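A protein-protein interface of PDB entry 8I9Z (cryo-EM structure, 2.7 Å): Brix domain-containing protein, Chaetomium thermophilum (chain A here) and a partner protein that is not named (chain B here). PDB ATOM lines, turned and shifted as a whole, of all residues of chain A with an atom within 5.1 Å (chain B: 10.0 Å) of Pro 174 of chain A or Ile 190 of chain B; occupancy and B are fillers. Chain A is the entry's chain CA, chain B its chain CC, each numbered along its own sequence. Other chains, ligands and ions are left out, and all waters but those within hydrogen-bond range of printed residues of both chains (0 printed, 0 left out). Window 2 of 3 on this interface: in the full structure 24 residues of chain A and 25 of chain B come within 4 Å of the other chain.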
ATOM      1  N   ILE A  27       3.856  10.565   6.867  1.00  0.00           N
ATOM      2  CA  ILE A  27       2.732  10.519   7.791  1.00  0.00           C
ATOM      3  C   ILE A  27       3.139  11.342   9.004  1.00  0.00           C
ATOM      4  O   ILE A  27       3.775  10.829   9.931  1.00  0.00           O
ATOM      5  CB  ILE A  27       2.354   9.090   8.188  1.00  0.00           C
ATOM      6  CG1 ILE A  27       2.119   8.233   6.951  1.00  0.00           C
ATOM      7  CG2 ILE A  27       1.106   9.096   9.045  1.00  0.00           C
ATOM      8  CD1 ILE A  27       2.239   6.761   7.214  1.00  0.00           C
ATOM      9  N   GLY A 168       7.876  11.606   9.430  1.00  0.00           N
ATOM     10  CA  GLY A 168       6.978  10.498   9.187  1.00  0.00           C
ATOM     11  C   GLY A 168       7.252   9.768   7.892  1.00  0.00           C
ATOM     12  O   GLY A 168       6.339   9.183   7.303  1.00  0.00           O
ATOM     13  N   HIS A 169       8.504   9.806   7.439  1.00  0.00           N
ATOM     14  CA  HIS A 169       8.864   9.231   6.149  1.00  0.00           C
ATOM     15  C   HIS A 169       8.707   7.715   6.173  1.00  0.00           C
ATOM     16  O   HIS A 169       9.149   7.048   7.111  1.00  0.00           O
ATOM     17  CB  HIS A 169      10.298   9.618   5.798  1.00  0.00           C
ATOM     18  CG  HIS A 169      10.568   9.683   4.329  1.00  0.00           C
ATOM     19  ND1 HIS A 169      10.931   8.580   3.588  1.00  0.00           N
ATOM     20  CD2 HIS A 169      10.528  10.721   3.462  1.00  0.00           C
ATOM     21  CE1 HIS A 169      11.099   8.936   2.328  1.00  0.00           C
ATOM     22  NE2 HIS A 169      10.863  10.231   2.226  1.00  0.00           N
ATOM     23  N   LYS A 170       8.075   7.173   5.133  1.00  0.00           N
ATOM     24  CA  LYS A 170       7.764   5.751   5.087  1.00  0.00           C
ATOM     25  C   LYS A 170       8.987   4.878   4.854  1.00  0.00           C
ATOM     26  O   LYS A 170       8.927   3.678   5.137  1.00  0.00           O
ATOM     27  CB  LYS A 170       6.729   5.474   4.002  1.00  0.00           C
ATOM     28  CG  LYS A 170       5.328   5.910   4.360  1.00  0.00           C
ATOM     29  CD  LYS A 170       4.366   5.577   3.248  1.00  0.00           C
ATOM     30  CE  LYS A 170       2.952   5.966   3.603  1.00  0.00           C
ATOM     31  NZ  LYS A 170       2.014   5.670   2.493  1.00  0.00           N
ATOM     32  N   SER A 172      11.872   5.475   6.409  1.00  0.00           N
ATOM     33  CA  SER A 172      12.747   5.676   7.548  1.00  0.00           C
ATOM     34  C   SER A 172      12.633   4.507   8.525  1.00  0.00           C
ATOM     35  O   SER A 172      11.862   3.566   8.324  1.00  0.00           O
ATOM     36  CB  SER A 172      12.425   7.005   8.225  1.00  0.00           C
ATOM     37  OG  SER A 172      11.096   7.021   8.706  1.00  0.00           O
ATOM     38  N   LYS A 173      13.422   4.562   9.599  1.00  0.00           N
ATOM     39  CA  LYS A 173      13.458   3.524  10.616  1.00  0.00           C
ATOM     40  C   LYS A 173      12.968   4.065  11.959  1.00  0.00           C
ATOM     41  O   LYS A 173      13.220   5.225  12.297  1.00  0.00           O
ATOM     42  CB  LYS A 173      14.875   2.960  10.780  1.00  0.00           C
ATOM     43  CG  LYS A 173      15.417   2.275   9.543  1.00  0.00           C
ATOM     44  CD  LYS A 173      14.740   0.949   9.309  1.00  0.00           C
ATOM     45  CE  LYS A 173      15.255   0.281   8.052  1.00  0.00           C
ATOM     46  NZ  LYS A 173      16.635  -0.224   8.226  1.00  0.00           N
ATOM     47  N   PRO A 174      12.272   3.246  12.751  1.00  0.00           N
ATOM     48  CA  PRO A 174      11.533   3.768  13.906  1.00  0.00           C
ATOM     49  C   PRO A 174      12.341   3.988  15.175  1.00  0.00           C
ATOM     50  O   PRO A 174      11.747   4.369  16.190  1.00  0.00           O
ATOM     51  CB  PRO A 174      10.471   2.689  14.135  1.00  0.00           C
ATOM     52  CG  PRO A 174      11.089   1.458  13.632  1.00  0.00           C
ATOM     53  CD  PRO A 174      11.910   1.850  12.460  1.00  0.00           C
ATOM     54  N   PHE A 175      13.650   3.770  15.186  1.00  0.00           N
ATOM     55  CA  PHE A 175      14.423   3.912  16.409  1.00  0.00           C
ATOM     56  C   PHE A 175      15.687   4.712  16.134  1.00  0.00           C
ATOM     57  O   PHE A 175      16.131   4.835  14.990  1.00  0.00           O
ATOM     58  CB  PHE A 175      14.753   2.540  17.007  1.00  0.00           C
ATOM     59  CG  PHE A 175      13.537   1.713  17.295  1.00  0.00           C
ATOM     60  CD1 PHE A 175      12.741   1.992  18.387  1.00  0.00           C
ATOM     61  CD2 PHE A 175      13.172   0.677  16.458  1.00  0.00           C
ATOM     62  CE1 PHE A 175      11.619   1.249  18.647  1.00  0.00           C
ATOM     63  CE2 PHE A 175      12.042  -0.067  16.714  1.00  0.00           C
ATOM     64  CZ  PHE A 175      11.266   0.224  17.810  1.00  0.00           C
ATOM     65  N   ILE A 176      16.261   5.267  17.197  1.00  0.00           N
ATOM     66  CA  ILE A 176      17.378   6.199  17.092  1.00  0.00           C
ATOM     67  C   ILE A 176      18.631   5.539  17.645  1.00  0.00           C
ATOM     68  O   ILE A 176      18.668   5.145  18.817  1.00  0.00           O
ATOM     69  CB  ILE A 176      17.075   7.510  17.826  1.00  0.00           C
ATOM     70  CG1 ILE A 176      15.859   8.174  17.176  1.00  0.00           C
ATOM     71  CG2 ILE A 176      18.308   8.403  17.836  1.00  0.00           C
ATOM     72  CD1 ILE A 176      15.782   9.654  17.339  1.00  0.00           C
ATOM     73  N   VAL B 167       5.845   2.238  -0.803  1.00  0.00           N
ATOM     74  CA  VAL B 167       6.788   1.828   0.233  1.00  0.00           C
ATOM     75  C   VAL B 167       6.107   0.782   1.102  1.00  0.00           C
ATOM     76  O   VAL B 167       4.978   1.009   1.551  1.00  0.00           O
ATOM     77  CB  VAL B 167       7.257   3.018   1.086  1.00  0.00           C
ATOM     78  CG1 VAL B 167       8.302   2.569   2.086  1.00  0.00           C
ATOM     79  CG2 VAL B 167       7.816   4.106   0.200  1.00  0.00           C
ATOM     80  N   PRO B 168       6.729  -0.371   1.337  1.00  0.00           N
ATOM     81  CA  PRO B 168       6.133  -1.360   2.235  1.00  0.00           C
ATOM     82  C   PRO B 168       6.094  -0.865   3.670  1.00  0.00           C
ATOM     83  O   PRO B 168       6.909  -0.043   4.094  1.00  0.00           O
ATOM     84  CB  PRO B 168       7.059  -2.573   2.091  1.00  0.00           C
ATOM     85  CG  PRO B 168       8.336  -2.013   1.594  1.00  0.00           C
ATOM     86  CD  PRO B 168       7.971  -0.860   0.724  1.00  0.00           C
ATOM     87  N   VAL B 169       5.117  -1.377   4.420  1.00  0.00           N
ATOM     88  CA  VAL B 169       4.927  -0.970   5.809  1.00  0.00           C
ATOM     89  C   VAL B 169       5.863  -1.690   6.767  1.00  0.00           C
ATOM     90  O   VAL B 169       5.940  -1.318   7.943  1.00  0.00           O
ATOM     91  CB  VAL B 169       3.444  -1.185   6.176  1.00  0.00           C
ATOM     92  CG1 VAL B 169       3.191  -2.626   6.570  1.00  0.00           C
ATOM     93  CG2 VAL B 169       2.991  -0.214   7.263  1.00  0.00           C
ATOM     94  N   ASN B 170       6.607  -2.689   6.292  1.00  0.00           N
ATOM     95  CA  ASN B 170       7.399  -3.536   7.175  1.00  0.00           C
ATOM     96  C   ASN B 170       8.667  -2.873   7.698  1.00  0.00           C
ATOM     97  O   ASN B 170       9.159  -3.291   8.750  1.00  0.00           O
ATOM     98  CB  ASN B 170       7.770  -4.835   6.467  1.00  0.00           C
ATOM     99  CG  ASN B 170       8.104  -5.945   7.438  1.00  0.00           C
ATOM    100  OD1 ASN B 170       7.800  -5.856   8.621  1.00  0.00           O
ATOM    101  ND2 ASN B 170       8.738  -6.997   6.941  1.00  0.00           N
ATOM    102  N   THR B 171       9.211  -1.881   6.984  1.00  0.00           N
ATOM    103  CA  THR B 171      10.474  -1.194   7.325  1.00  0.00           C
ATOM    104  C   THR B 171      11.629  -2.171   7.547  1.00  0.00           C
ATOM    105  O   THR B 171      12.518  -1.931   8.362  1.00  0.00           O
ATOM    106  CB  THR B 171      10.326  -0.276   8.541  1.00  0.00           C
ATOM    107  OG1 THR B 171      10.364  -1.057   9.740  1.00  0.00           O
ATOM    108  CG2 THR B 171       9.024   0.500   8.476  1.00  0.00           C
ATOM    109  N   ILE B 172      11.621  -3.278   6.819  1.00  0.00           N
ATOM    110  CA  ILE B 172      12.659  -4.294   6.894  1.00  0.00           C
ATOM    111  C   ILE B 172      13.360  -4.306   5.545  1.00  0.00           C
ATOM    112  O   ILE B 172      12.705  -4.431   4.503  1.00  0.00           O
ATOM    113  CB  ILE B 172      12.074  -5.674   7.238  1.00  0.00           C
ATOM    114  CG1 ILE B 172      11.463  -5.660   8.637  1.00  0.00           C
ATOM    115  CG2 ILE B 172      13.117  -6.747   7.143  1.00  0.00           C
ATOM    116  CD1 ILE B 172      12.375  -5.108   9.696  1.00  0.00           C
ATOM    117  N   GLY B 173      14.679  -4.165   5.561  1.00  0.00           N
ATOM    118  CA  GLY B 173      15.421  -3.996   4.330  1.00  0.00           C
ATOM    119  C   GLY B 173      15.653  -5.280   3.567  1.00  0.00           C
ATOM    120  O   GLY B 173      14.769  -6.135   3.487  1.00  0.00           O
ATOM    121  N   TYR B 180      13.119 -13.791  11.669  1.00  0.00           N
ATOM    122  CA  TYR B 180      11.833 -13.713  12.334  1.00  0.00           C
ATOM    123  C   TYR B 180      11.093 -15.037  12.346  1.00  0.00           C
ATOM    124  O   TYR B 180       9.876 -15.039  12.563  1.00  0.00           O
ATOM    125  CB  TYR B 180      10.944 -12.667  11.652  1.00  0.00           C
ATOM    126  CG  TYR B 180      11.380 -11.239  11.841  1.00  0.00           C
ATOM    127  CD1 TYR B 180      11.167 -10.576  13.038  1.00  0.00           C
ATOM    128  CD2 TYR B 180      11.991 -10.548  10.811  1.00  0.00           C
ATOM    129  CE1 TYR B 180      11.561  -9.269  13.202  1.00  0.00           C
ATOM    130  CE2 TYR B 180      12.387  -9.244  10.968  1.00  0.00           C
ATOM    131  CZ  TYR B 180      12.169  -8.611  12.163  1.00  0.00           C
ATOM    132  OH  TYR B 180      12.568  -7.309  12.315  1.00  0.00           O
ATOM    133  N   ILE B 186       6.501  -9.865  12.717  1.00  0.00           N
ATOM    134  CA  ILE B 186       7.346  -9.753  11.531  1.00  0.00           C
ATOM    135  C   ILE B 186       7.606  -8.262  11.287  1.00  0.00           C
ATOM    136  O   ILE B 186       6.756  -7.516  10.792  1.00  0.00           O
ATOM    137  CB  ILE B 186       6.753 -10.497  10.317  1.00  0.00           C
ATOM    138  CG1 ILE B 186       7.815 -10.874   9.281  1.00  0.00           C
ATOM    139  CG2 ILE B 186       5.381  -9.984   9.776  1.00  0.00           C
ATOM    140  CD1 ILE B 186       7.221 -11.422   8.000  1.00  0.00           C
ATOM    141  N   GLY B 187       8.764  -7.791  11.741  1.00  0.00           N
ATOM    142  CA  GLY B 187       9.156  -6.411  11.538  1.00  0.00           C
ATOM    143  C   GLY B 187       8.436  -5.410  12.428  1.00  0.00           C
ATOM    144  O   GLY B 187       7.535  -5.730  13.204  1.00  0.00           O
ATOM    145  N   TYR B 188       8.861  -4.154  12.293  1.00  0.00           N
ATOM    146  CA  TYR B 188       8.284  -3.012  12.987  1.00  0.00           C
ATOM    147  C   TYR B 188       7.917  -1.946  11.966  1.00  0.00           C
ATOM    148  O   TYR B 188       8.639  -1.743  10.993  1.00  0.00           O
ATOM    149  CB  TYR B 188       9.269  -2.396  13.990  1.00  0.00           C
ATOM    150  CG  TYR B 188       9.372  -3.077  15.330  1.00  0.00           C
ATOM    151  CD1 TYR B 188       9.995  -4.307  15.461  1.00  0.00           C
ATOM    152  CD2 TYR B 188       8.881  -2.470  16.471  1.00  0.00           C
ATOM    153  CE1 TYR B 188      10.105  -4.920  16.682  1.00  0.00           C
ATOM    154  CE2 TYR B 188       8.986  -3.077  17.698  1.00  0.00           C
ATOM    155  CZ  TYR B 188       9.598  -4.303  17.796  1.00  0.00           C
ATOM    156  OH  TYR B 188       9.703  -4.908  19.023  1.00  0.00           O
ATOM    157  N   ASP B 189       6.813  -1.241  12.195  1.00  0.00           N
ATOM    158  CA  ASP B 189       6.481  -0.135  11.309  1.00  0.00           C
ATOM    159  C   ASP B 189       7.242   1.120  11.738  1.00  0.00           C
ATOM    160  O   ASP B 189       8.027   1.097  12.685  1.00  0.00           O
ATOM    161  CB  ASP B 189       4.966   0.089  11.254  1.00  0.00           C
ATOM    162  CG  ASP B 189       4.325   0.271  12.622  1.00  0.00           C
ATOM    163  OD1 ASP B 189       5.012   0.632  13.598  1.00  0.00           O
ATOM    164  OD2 ASP B 189       3.101   0.048  12.718  1.00  0.00           O
ATOM    165  N   ILE B 190       6.994   2.237  11.048  1.00  0.00           N
ATOM    166  CA  ILE B 190       7.761   3.456  11.287  1.00  0.00           C
ATOM    167  C   ILE B 190       7.473   4.076  12.647  1.00  0.00           C
ATOM    168  O   ILE B 190       8.266   4.892  13.127  1.00  0.00           O
ATOM    169  CB  ILE B 190       7.499   4.500  10.187  1.00  0.00           C
ATOM    170  CG1 ILE B 190       6.003   4.775  10.057  1.00  0.00           C
ATOM    171  CG2 ILE B 190       8.071   4.047   8.867  1.00  0.00           C
ATOM    172  CD1 ILE B 190       5.678   5.956   9.182  1.00  0.00           C
ATOM    173  N   ASN B 191       6.356   3.729  13.277  1.00  0.00           N
ATOM    174  CA  ASN B 191       6.011   4.318  14.561  1.00  0.00           C
ATOM    175  C   ASN B 191       6.617   3.573  15.738  1.00  0.00           C
ATOM    176  O   ASN B 191       6.533   4.062  16.868  1.00  0.00           O
ATOM    177  CB  ASN B 191       4.493   4.373  14.716  1.00  0.00           C
ATOM    178  CG  ASN B 191       3.898   5.630  14.130  1.00  0.00           C
ATOM    179  OD1 ASN B 191       4.281   6.061  13.045  1.00  0.00           O
ATOM    180  ND2 ASN B 191       2.953   6.227  14.844  1.00  0.00           N
ATOM    181  N   GLY B 192       7.222   2.412  15.510  1.00  0.00           N
ATOM    182  CA  GLY B 192       7.869   1.665  16.564  1.00  0.00           C
ATOM    183  C   GLY B 192       7.069   0.526  17.152  1.00  0.00           C
ATOM    184  O   GLY B 192       7.521  -0.076  18.132  1.00  0.00           O
ATOM    185  N   LYS B 193       5.901   0.212  16.601  1.00  0.00           N
ATOM    186  CA  LYS B 193       5.108  -0.917  17.066  1.00  0.00           C
ATOM    187  C   LYS B 193       5.256  -2.074  16.087  1.00  0.00           C
ATOM    188  O   LYS B 193       5.281  -1.869  14.870  1.00  0.00           O
ATOM    189  CB  LYS B 193       3.639  -0.528  17.250  1.00  0.00           C
ATOM    190  CG  LYS B 193       2.941   0.046  16.028  1.00  0.00           C
ATOM    191  CD  LYS B 193       1.422   0.193  16.209  1.00  0.00           C
ATOM    192  CE  LYS B 193       0.841  -0.745  17.265  1.00  0.00           C
ATOM    193  NZ  LYS B 193      -0.637  -0.607  17.389  1.00  0.00           N
ATOM    194  N   LYS B 194       5.375  -3.281  16.622  1.00  0.00           N
ATOM    195  CA  LYS B 194       5.647  -4.442  15.792  1.00  0.00           C
ATOM    196  C   LYS B 194       4.423  -4.837  14.975  1.00  0.00           C
ATOM    197  O   LYS B 194       3.278  -4.609  15.371  1.00  0.00           O
ATOM    198  CB  LYS B 194       6.105  -5.615  16.657  1.00  0.00           C
ATOM    199  CG  LYS B 194       5.177  -5.929  17.808  1.00  0.00           C
ATOM    200  CD  LYS B 194       5.693  -7.097  18.622  1.00  0.00           C
ATOM    201  CE  LYS B 194       6.944  -6.725  19.389  1.00  0.00           C
ATOM    202  NZ  LYS B 194       7.398  -7.843  20.254  1.00  0.00           N
ATOM    203  N   ILE B 195       4.686  -5.431  13.816  1.00  0.00           N
ATOM    204  CA  ILE B 195       3.653  -5.889  12.897  1.00  0.00           C
ATOM    205  C   ILE B 195       3.437  -7.372  13.140  1.00  0.00           C
ATOM    206  O   ILE B 195       4.370  -8.172  13.015  1.00  0.00           O
ATOM    207  CB  ILE B 195       4.046  -5.621  11.437  1.00  0.00           C
ATOM    208  CG1 ILE B 195       4.265  -4.130  11.221  1.00  0.00           C
ATOM    209  CG2 ILE B 195       2.984  -6.144  10.496  1.00  0.00           C
ATOM    210  CD1 ILE B 195       4.874  -3.811   9.900  1.00  0.00           C
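Printed residues of chain B within 4 Å of Gly 168 of chain A: Ile 190 (3.8 Å).
Of the printed residues of chain B, Lys 170 of chain A touches Val 167 and Ile 190.
Ser 172 of chain A touches one residue of chain B.
Of the printed residues of chain B, Lys 173 of chain A touches Thr 171.
Pro 174 of chain A touches three residues of chain B.
Of the printed residues of chain A, Thr 171 of chain B touches Lys 173 (3.5 Å).
Printed residues of chain A within 4 Å of Asp 189 of chain B: Pro 174 (3.2 Å).
Ile 190 of chain B touches five residues of chain A.
Lys 193 of chain B touches none of the printed residues of chain A.
The nearest residue of chain A that does not touch Ile 190 of chain B is Ile 27 of chain A (4.04 Å).
The nearest printed residue of chain B that does not touch His 169 of chain A is Val 167 of chain B (6.2 Å).
The backbone carbonyl oxygen (O) of Gly 168 of chain A lies within hydrogen-bond range of the backbone NH (N) of Ile 27 of chain A (2.9 Å).
The backbone carbonyl oxygen (O) of His 169 of chain A is in hydrogen-bond range of the side-chain hydroxyl (OG) of Ser 172 of chain A.
The backbone NH (N) of Asn 191 of chain B sits close to the side-chain carboxylate (OD1) of Asp 189 of chain B (3.4 Å).
The side-chain carboxylate of Asp 189 of chain B is in hydrogen-bond range of the backbone NH of Gly 192 of chain B.
N of Lys 193 of chain B sits at hydrogen-bond distance from OD1 of Asp 189 of chain B.
Gly 168 of chain A touches Ile 190 of chain B.
His 169 of chain A touches Ile 190 of chain B.
Lys 170 of chain A touches Val 167 of chain B.
Ile 190 of chain B touches Lys 170 of chain A (CG2 to O, 3.8 Å).
O of Ser 172 of chain A touches CG2 of Ile 190 of chain B (3.9 Å).
CE of Lys 173 of chain A touches O of Thr 171 of chain B, at 3.5 Å.
Pro 174 of chain A touches Asp 189 of chain B (CG to O, 3.2 Å).
Pro 174 of chain A touches Ile 190 of chain B (CB to O, 3.3 Å).
Phe 175 of chain A touches Tyr 188 of chain B.
CZ of Phe 175 of chain A touches O of Gly 192 of chain B, at 3.8 Å.
Hydrophobic or aromatic side chains of chain A that line the printed part of chain B: Pro 174 and Phe 175.
Along chain A the printed residues that touch a printed residue of chain B span positions 168 to 175.
Of the 18 printed residues of chain B, 6 touch a printed residue of chain A.
Among the printed residues, 11 pairs touch across the chains.
Among the printed residues, no Asp or Glu carboxylate lies within 4 Å of a Lys or Arg side-chain nitrogen of the other chain.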
